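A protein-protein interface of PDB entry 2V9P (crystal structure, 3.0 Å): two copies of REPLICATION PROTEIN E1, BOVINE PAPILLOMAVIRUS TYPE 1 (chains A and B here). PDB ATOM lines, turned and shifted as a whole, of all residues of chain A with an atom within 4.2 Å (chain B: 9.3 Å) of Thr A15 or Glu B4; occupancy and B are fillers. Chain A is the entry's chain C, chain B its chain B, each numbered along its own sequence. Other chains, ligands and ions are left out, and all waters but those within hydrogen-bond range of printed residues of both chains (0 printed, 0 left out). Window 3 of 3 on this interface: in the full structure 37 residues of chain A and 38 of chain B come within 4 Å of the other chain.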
ATOM      1  N   ASP A  12       3.008  26.866 -15.673  1.00  0.00           N
ATOM      2  CA  ASP A  12       1.633  26.394 -15.485  1.00  0.00           C
ATOM      3  C   ASP A  12       0.676  27.299 -16.228  1.00  0.00           C
ATOM      4  O   ASP A  12       0.639  28.502 -15.970  1.00  0.00           O
ATOM      5  CB  ASP A  12       1.229  26.347 -14.010  1.00  0.00           C
ATOM      6  CG  ASP A  12      -0.237  25.935 -13.817  1.00  0.00           C
ATOM      7  OD1 ASP A  12      -0.578  24.782 -14.157  1.00  0.00           O
ATOM      8  OD2 ASP A  12      -1.048  26.758 -13.335  1.00  0.00           O
ATOM      9  N   PHE A  13      -0.107  26.710 -17.130  1.00  0.00           N
ATOM     10  CA  PHE A  13      -1.059  27.460 -17.947  1.00  0.00           C
ATOM     11  C   PHE A  13      -2.109  28.120 -17.071  1.00  0.00           C
ATOM     12  O   PHE A  13      -2.306  29.328 -17.137  1.00  0.00           O
ATOM     13  CB  PHE A  13      -1.707  26.531 -18.981  1.00  0.00           C
ATOM     14  CG  PHE A  13      -2.691  27.213 -19.902  1.00  0.00           C
ATOM     15  CD1 PHE A  13      -2.262  28.127 -20.865  1.00  0.00           C
ATOM     16  CD2 PHE A  13      -4.049  26.909 -19.836  1.00  0.00           C
ATOM     17  CE1 PHE A  13      -3.182  28.759 -21.736  1.00  0.00           C
ATOM     18  CE2 PHE A  13      -4.970  27.525 -20.704  1.00  0.00           C
ATOM     19  CZ  PHE A  13      -4.529  28.458 -21.651  1.00  0.00           C
ATOM     20  N   GLY A  14      -2.748  27.317 -16.228  1.00  0.00           N
ATOM     21  CA  GLY A  14      -3.813  27.783 -15.343  1.00  0.00           C
ATOM     22  C   GLY A  14      -3.537  29.077 -14.601  1.00  0.00           C
ATOM     23  O   GLY A  14      -4.427  29.914 -14.453  1.00  0.00           O
ATOM     24  N   THR A  15      -2.302  29.231 -14.130  1.00  0.00           N
ATOM     25  CA  THR A  15      -1.870  30.426 -13.404  1.00  0.00           C
ATOM     26  C   THR A  15      -1.887  31.649 -14.301  1.00  0.00           C
ATOM     27  O   THR A  15      -2.285  32.737 -13.869  1.00  0.00           O
ATOM     28  CB  THR A  15      -0.456  30.253 -12.862  1.00  0.00           C
ATOM     29  OG1 THR A  15      -0.343  28.965 -12.255  1.00  0.00           O
ATOM     30  CG2 THR A  15      -0.124  31.351 -11.854  1.00  0.00           C
ATOM     31  N   MET A  16      -1.436  31.465 -15.541  1.00  0.00           N
ATOM     32  CA  MET A  16      -1.508  32.519 -16.528  1.00  0.00           C
ATOM     33  C   MET A  16      -2.957  32.923 -16.782  1.00  0.00           C
ATOM     34  O   MET A  16      -3.276  34.108 -16.852  1.00  0.00           O
ATOM     35  CB  MET A  16      -0.860  32.104 -17.842  1.00  0.00           C
ATOM     36  CG  MET A  16      -1.179  33.097 -18.955  1.00  0.00           C
ATOM     37  SD  MET A  16       0.035  33.130 -20.257  1.00  0.00           S
ATOM     38  CE  MET A  16      -0.719  32.028 -21.414  1.00  0.00           C
ATOM     39  N   VAL A  17      -3.826  31.931 -16.924  1.00  0.00           N
ATOM     40  CA  VAL A  17      -5.243  32.197 -17.145  1.00  0.00           C
ATOM     41  C   VAL A  17      -5.808  32.931 -15.944  1.00  0.00           C
ATOM     42  O   VAL A  17      -6.460  33.963 -16.086  1.00  0.00           O
ATOM     43  CB  VAL A  17      -6.049  30.911 -17.375  1.00  0.00           C
ATOM     44  CG1 VAL A  17      -7.375  31.242 -18.004  1.00  0.00           C
ATOM     45  CG2 VAL A  17      -5.287  29.974 -18.272  1.00  0.00           C
ATOM     46  N   GLN A  18      -5.540  32.394 -14.760  1.00  0.00           N
ATOM     47  CA  GLN A  18      -5.969  33.015 -13.526  1.00  0.00           C
ATOM     48  C   GLN A  18      -5.643  34.498 -13.588  1.00  0.00           C
ATOM     49  O   GLN A  18      -6.512  35.348 -13.389  1.00  0.00           O
ATOM     50  CB  GLN A  18      -5.270  32.356 -12.329  1.00  0.00           C
ATOM     51  CG  GLN A  18      -5.760  32.856 -10.987  1.00  0.00           C
ATOM     52  CD  GLN A  18      -7.198  32.477 -10.740  1.00  0.00           C
ATOM     53  OE1 GLN A  18      -7.491  31.333 -10.398  1.00  0.00           O
ATOM     54  NE2 GLN A  18      -8.108  33.429 -10.924  1.00  0.00           N
ATOM     55  N   TRP A  19      -4.378  34.785 -13.885  1.00  0.00           N
ATOM     56  CA  TRP A  19      -3.875  36.144 -13.960  1.00  0.00           C
ATOM     57  C   TRP A  19      -4.733  36.930 -14.944  1.00  0.00           C
ATOM     58  O   TRP A  19      -5.366  37.919 -14.567  1.00  0.00           O
ATOM     59  CB  TRP A  19      -2.391  36.127 -14.359  1.00  0.00           C
ATOM     60  CG  TRP A  19      -1.806  37.461 -14.740  1.00  0.00           C
ATOM     61  CD1 TRP A  19      -1.253  38.383 -13.899  1.00  0.00           C
ATOM     62  CD2 TRP A  19      -1.695  38.010 -16.066  1.00  0.00           C
ATOM     63  NE1 TRP A  19      -0.810  39.475 -14.611  1.00  0.00           N
ATOM     64  CE2 TRP A  19      -1.071  39.274 -15.943  1.00  0.00           C
ATOM     65  CE3 TRP A  19      -2.064  37.556 -17.348  1.00  0.00           C
ATOM     66  CZ2 TRP A  19      -0.811  40.094 -17.051  1.00  0.00           C
ATOM     67  CZ3 TRP A  19      -1.803  38.371 -18.447  1.00  0.00           C
ATOM     68  CH2 TRP A  19      -1.179  39.626 -18.288  1.00  0.00           C
ATOM     69  N   ASN A  44       6.242  32.363 -12.878  1.00  0.00           N
ATOM     70  CA  ASN A  44       5.426  31.763 -13.925  1.00  0.00           C
ATOM     71  C   ASN A  44       5.461  32.565 -15.224  1.00  0.00           C
ATOM     72  O   ASN A  44       5.388  31.993 -16.312  1.00  0.00           O
ATOM     73  CB  ASN A  44       3.982  31.580 -13.461  1.00  0.00           C
ATOM     74  CG  ASN A  44       3.180  30.708 -14.404  1.00  0.00           C
ATOM     75  OD1 ASN A  44       3.594  29.599 -14.748  1.00  0.00           O
ATOM     76  ND2 ASN A  44       2.029  31.205 -14.832  1.00  0.00           N
ATOM     77  N   THR B   1     -13.863  33.564  -9.276  1.00  0.00           N
ATOM     78  CA  THR B   1     -13.570  32.270  -9.962  1.00  0.00           C
ATOM     79  C   THR B   1     -12.103  31.871  -9.708  1.00  0.00           C
ATOM     80  O   THR B   1     -11.234  32.737  -9.508  1.00  0.00           O
ATOM     81  CB  THR B   1     -13.968  32.307 -11.516  1.00  0.00           C
ATOM     82  OG1 THR B   1     -14.578  31.073 -11.927  1.00  0.00           O
ATOM     83  CG2 THR B   1     -12.787  32.565 -12.414  1.00  0.00           C
ATOM     84  N   LEU B   2     -11.859  30.557  -9.666  1.00  0.00           N
ATOM     85  CA  LEU B   2     -10.508  29.999  -9.669  1.00  0.00           C
ATOM     86  C   LEU B   2     -10.303  29.114 -10.892  1.00  0.00           C
ATOM     87  O   LEU B   2     -11.109  28.220 -11.162  1.00  0.00           O
ATOM     88  CB  LEU B   2     -10.240  29.174  -8.413  1.00  0.00           C
ATOM     89  CG  LEU B   2      -9.811  29.860  -7.123  1.00  0.00           C
ATOM     90  CD1 LEU B   2      -9.424  28.772  -6.130  1.00  0.00           C
ATOM     91  CD2 LEU B   2      -8.644  30.834  -7.334  1.00  0.00           C
ATOM     92  N   ASN B   3      -9.222  29.367 -11.622  1.00  0.00           N
ATOM     93  CA  ASN B   3      -8.836  28.541 -12.763  1.00  0.00           C
ATOM     94  C   ASN B   3      -7.454  27.952 -12.517  1.00  0.00           C
ATOM     95  O   ASN B   3      -6.914  27.254 -13.375  1.00  0.00           O
ATOM     96  CB  ASN B   3      -8.793  29.380 -14.036  1.00  0.00           C
ATOM     97  CG  ASN B   3      -9.500  30.701 -13.876  1.00  0.00           C
ATOM     98  OD1 ASN B   3     -10.725  30.757 -13.867  1.00  0.00           O
ATOM     99  ND2 ASN B   3      -8.730  31.773 -13.734  1.00  0.00           N
ATOM    100  N   GLU B   4      -6.886  28.239 -11.346  1.00  0.00           N
ATOM    101  CA  GLU B   4      -5.533  27.811 -11.034  1.00  0.00           C
ATOM    102  C   GLU B   4      -5.537  26.511 -10.226  1.00  0.00           C
ATOM    103  O   GLU B   4      -6.464  25.713 -10.344  1.00  0.00           O
ATOM    104  CB  GLU B   4      -4.798  28.927 -10.295  1.00  0.00           C
ATOM    105  CG  GLU B   4      -3.297  28.894 -10.504  1.00  0.00           C
ATOM    106  CD  GLU B   4      -2.544  29.792  -9.542  1.00  0.00           C
ATOM    107  OE1 GLU B   4      -2.816  31.017  -9.544  1.00  0.00           O
ATOM    108  OE2 GLU B   4      -1.671  29.273  -8.795  1.00  0.00           O
ATOM    109  N   SER B   5      -4.487  26.302  -9.428  1.00  0.00           N
ATOM    110  CA  SER B   5      -4.355  25.147  -8.528  1.00  0.00           C
ATOM    111  C   SER B   5      -3.493  25.497  -7.313  1.00  0.00           C
ATOM    112  O   SER B   5      -2.437  26.124  -7.450  1.00  0.00           O
ATOM    113  CB  SER B   5      -3.756  23.943  -9.265  1.00  0.00           C
ATOM    114  OG  SER B   5      -4.596  23.533 -10.333  1.00  0.00           O
ATOM    115  N   ALA B  36     -14.688  24.500 -14.484  1.00  0.00           N
ATOM    116  CA  ALA B  36     -13.719  25.197 -13.648  1.00  0.00           C
ATOM    117  C   ALA B  36     -14.355  25.519 -12.309  1.00  0.00           C
ATOM    118  O   ALA B  36     -13.662  25.663 -11.300  1.00  0.00           O
ATOM    119  CB  ALA B  36     -13.228  26.464 -14.324  1.00  0.00           C
ATOM    120  N   LEU B  37     -15.679  25.620 -12.305  1.00  0.00           N
ATOM    121  CA  LEU B  37     -16.411  25.822 -11.069  1.00  0.00           C
ATOM    122  C   LEU B  37     -16.492  24.530 -10.276  1.00  0.00           C
ATOM    123  O   LEU B  37     -16.225  24.522  -9.067  1.00  0.00           O
ATOM    124  CB  LEU B  37     -17.805  26.395 -11.326  1.00  0.00           C
ATOM    125  CG  LEU B  37     -17.824  27.900 -11.589  1.00  0.00           C
ATOM    126  CD1 LEU B  37     -19.194  28.367 -12.025  1.00  0.00           C
ATOM    127  CD2 LEU B  37     -17.344  28.685 -10.372  1.00  0.00           C
ATOM    128  N   ALA B  39     -14.503  22.523  -9.918  1.00  0.00           N
ATOM    129  CA  ALA B  39     -13.144  22.232  -9.441  1.00  0.00           C
ATOM    130  C   ALA B  39     -12.961  22.205  -7.925  1.00  0.00           C
ATOM    131  O   ALA B  39     -12.032  21.565  -7.429  1.00  0.00           O
ATOM    132  CB  ALA B  39     -12.143  23.185 -10.072  1.00  0.00           C
ATOM    133  N   GLY B  40     -13.836  22.900  -7.199  1.00  0.00           N
ATOM    134  CA  GLY B  40     -13.746  22.985  -5.739  1.00  0.00           C
ATOM    135  C   GLY B  40     -14.026  21.661  -5.048  1.00  0.00           C
ATOM    136  O   GLY B  40     -13.429  21.345  -4.017  1.00  0.00           O
ATOM    137  N   ALA B  45     -12.044  17.877 -12.138  1.00  0.00           N
ATOM    138  CA  ALA B  45     -12.087  19.270 -12.555  1.00  0.00           C
ATOM    139  C   ALA B  45     -10.830  19.990 -12.091  1.00  0.00           C
ATOM    140  O   ALA B  45     -10.289  20.837 -12.801  1.00  0.00           O
ATOM    141  CB  ALA B  45     -13.336  19.947 -12.032  1.00  0.00           C
ATOM    142  N   ARG B  46     -10.365  19.633 -10.899  1.00  0.00           N
ATOM    143  CA  ARG B  46      -9.082  20.100 -10.385  1.00  0.00           C
ATOM    144  C   ARG B  46      -7.941  19.696 -11.325  1.00  0.00           C
ATOM    145  O   ARG B  46      -7.101  20.527 -11.673  1.00  0.00           O
ATOM    146  CB  ARG B  46      -8.843  19.512  -8.994  1.00  0.00           C
ATOM    147  CG  ARG B  46      -8.053  20.396  -8.027  1.00  0.00           C
ATOM    148  CD  ARG B  46      -8.121  19.840  -6.596  1.00  0.00           C
ATOM    149  NE  ARG B  46      -9.372  19.105  -6.375  1.00  0.00           N
ATOM    150  CZ  ARG B  46      -9.743  18.528  -5.233  1.00  0.00           C
ATOM    151  NH1 ARG B  46      -8.970  18.592  -4.156  1.00  0.00           N
ATOM    152  NH2 ARG B  46     -10.903  17.887  -5.169  1.00  0.00           N
ATOM    153  N   ALA B  47      -7.935  18.424 -11.740  1.00  0.00           N
ATOM    154  CA  ALA B  47      -6.899  17.860 -12.612  1.00  0.00           C
ATOM    155  C   ALA B  47      -6.884  18.542 -13.972  1.00  0.00           C
ATOM    156  O   ALA B  47      -5.822  18.708 -14.587  1.00  0.00           O
ATOM    157  CB  ALA B  47      -7.106  16.360 -12.776  1.00  0.00           C
ATOM    158  N   PHE B  48      -8.079  18.928 -14.421  1.00  0.00           N
ATOM    159  CA  PHE B  48      -8.297  19.632 -15.682  1.00  0.00           C
ATOM    160  C   PHE B  48      -7.591  20.988 -15.703  1.00  0.00           C
ATOM    161  O   PHE B  48      -7.013  21.391 -16.713  1.00  0.00           O
ATOM    162  CB  PHE B  48      -9.804  19.795 -15.914  1.00  0.00           C
ATOM    163  CG  PHE B  48     -10.163  20.829 -16.939  1.00  0.00           C
ATOM    164  CD1 PHE B  48     -10.168  20.514 -18.289  1.00  0.00           C
ATOM    165  CD2 PHE B  48     -10.507  22.117 -16.548  1.00  0.00           C
ATOM    166  CE1 PHE B  48     -10.498  21.463 -19.229  1.00  0.00           C
ATOM    167  CE2 PHE B  48     -10.838  23.075 -17.483  1.00  0.00           C
ATOM    168  CZ  PHE B  48     -10.833  22.747 -18.823  1.00  0.00           C
ATOM    169  N   LEU B  49      -7.633  21.687 -14.581  1.00  0.00           N
ATOM    170  CA  LEU B  49      -6.943  22.954 -14.472  1.00  0.00           C
ATOM    171  C   LEU B  49      -5.426  22.781 -14.289  1.00  0.00           C
ATOM    172  O   LEU B  49      -4.685  23.759 -14.363  1.00  0.00           O
ATOM    173  CB  LEU B  49      -7.546  23.784 -13.342  1.00  0.00           C
ATOM    174  CG  LEU B  49      -9.050  24.064 -13.426  1.00  0.00           C
ATOM    175  CD1 LEU B  49      -9.567  24.523 -12.094  1.00  0.00           C
ATOM    176  CD2 LEU B  49      -9.374  25.105 -14.473  1.00  0.00           C
ATOM    177  N   ALA B  50      -4.975  21.546 -14.063  1.00  0.00           N
ATOM    178  CA  ALA B  50      -3.542  21.250 -13.972  1.00  0.00           C
ATOM    179  C   ALA B  50      -2.889  20.966 -15.335  1.00  0.00           C
ATOM    180  O   ALA B  50      -1.658  21.115 -15.480  1.00  0.00           O
ATOM    181  CB  ALA B  50      -3.275  20.098 -12.993  1.00  0.00           C
ATOM    182  N   THR B  51      -3.703  20.555 -16.318  1.00  0.00           N
ATOM    183  CA  THR B  51      -3.201  20.260 -17.674  1.00  0.00           C
ATOM    184  C   THR B  51      -2.970  21.525 -18.479  1.00  0.00           C
ATOM    185  O   THR B  51      -3.697  22.507 -18.342  1.00  0.00           O
ATOM    186  CB  THR B  51      -4.153  19.371 -18.516  1.00  0.00           C
ATOM    187  OG1 THR B  51      -5.504  19.805 -18.323  1.00  0.00           O
ATOM    188  CG2 THR B  51      -4.022  17.894 -18.151  1.00  0.00           C
ATOM    189  N   ASN B  52      -1.956  21.466 -19.336  1.00  0.00           N
ATOM    190  CA  ASN B  52      -1.588  22.565 -20.208  1.00  0.00           C
ATOM    191  C   ASN B  52      -2.376  22.566 -21.514  1.00  0.00           C
ATOM    192  O   ASN B  52      -2.261  23.484 -22.313  1.00  0.00           O
ATOM    193  CB  ASN B  52      -0.090  22.499 -20.491  1.00  0.00           C
ATOM    194  CG  ASN B  52       0.728  22.677 -19.241  1.00  0.00           C
ATOM    195  OD1 ASN B  52       0.803  23.784 -18.702  1.00  0.00           O
ATOM    196  ND2 ASN B  52       1.330  21.584 -18.746  1.00  0.00           N
ATOM    197  N   GLN B  54      -5.792  22.295 -21.700  1.00  0.00           N
ATOM    198  CA  GLN B  54      -7.199  22.429 -21.311  1.00  0.00           C
ATOM    199  C   GLN B  54      -8.028  23.030 -22.412  1.00  0.00           C
ATOM    200  O   GLN B  54      -9.191  22.691 -22.566  1.00  0.00           O
ATOM    201  CB  GLN B  54      -7.387  23.224 -20.019  1.00  0.00           C
ATOM    202  CG  GLN B  54      -6.225  24.087 -19.622  1.00  0.00           C
ATOM    203  CD  GLN B  54      -6.461  24.817 -18.306  1.00  0.00           C
ATOM    204  OE1 GLN B  54      -7.268  25.747 -18.244  1.00  0.00           O
ATOM    205  NE2 GLN B  54      -5.738  24.408 -17.248  1.00  0.00           N
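N of Asn B3 sits at hydrogen-bond distance from OE1 of Gln A18 (2.9 Å). OE1 of Gln A18 lies within hydrogen-bond range of N of Glu B4 (3.3 Å). The side-chain amide oxygen (OD1) of Asn B52 sits at hydrogen-bond distance from the backbone NH (N) of Phe A13, 3.4 Å away.
NE2 of Gln B54 sits at hydrogen-bond distance from O of Phe B48. O of Leu B49 sits at hydrogen-bond distance from NE2 of Gln B54 (3.1 Å). The backbone carbonyl oxygen (O) of Thr B51 sits at hydrogen-bond distance from the side-chain amide nitrogen (NE2) of Gln B54 (3.0 Å). The side-chain carboxylate (OD2) of Asp A12 sits at hydrogen-bond distance from the backbone NH (N) of Gly A14 (3.4 Å). OG1 of Thr A15 sits at hydrogen-bond distance from OD2 of Asp A12, at 2.6 Å.
Among the printed residues, pairs that only touch across the chains: Phe A13 with Gln B54, Gly A14 with Asn B3, Thr A15 with Glu B4, Val A17 with Asn B3, Gln A18 with Thr B1 and Gln A18 with Leu B2.
No residue of chain B comes within 4 Å of Asp A12. Of the printed residues of chain B, Phe A13 touches Asn B52 and Gln B54. Printed residues of chain B within 4 Å of Gly A14: Asn B3. Thr A15 touches just one residue of chain B: Glu B4. Printed residues of chain B within 4 Å of Val A17: Asn B3. Of the printed residues of chain B, Gln A18 touches Thr B1, Leu B2, Asn B3 and Glu B4. Printed residues of chain A within 4 Å of Thr B1: Gln A18 (3.5 Å). Of the printed residues of chain A, Asn B3 touches Gly A14, Val A17 and Gln A18. Of chain A, only Thr A15 (3.4 Å) and Gln A18 (3.3 Å) come within 4 Å of Glu B4. The nearest printed residue of chain A that does not touch Asn B3 is Thr A15 (5.1 Å).
Printed residues of chain A that touch a printed residue of chain B: Phe A13, Gly A14, Thr A15, Val A17 and Gln A18. Hydrophobic or aromatic side chains of chain A within 4 Å of the printed part of chain B: Phe A13. Among the printed residues, 9 pairs touch across the chains.
No position is printed for both chains.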
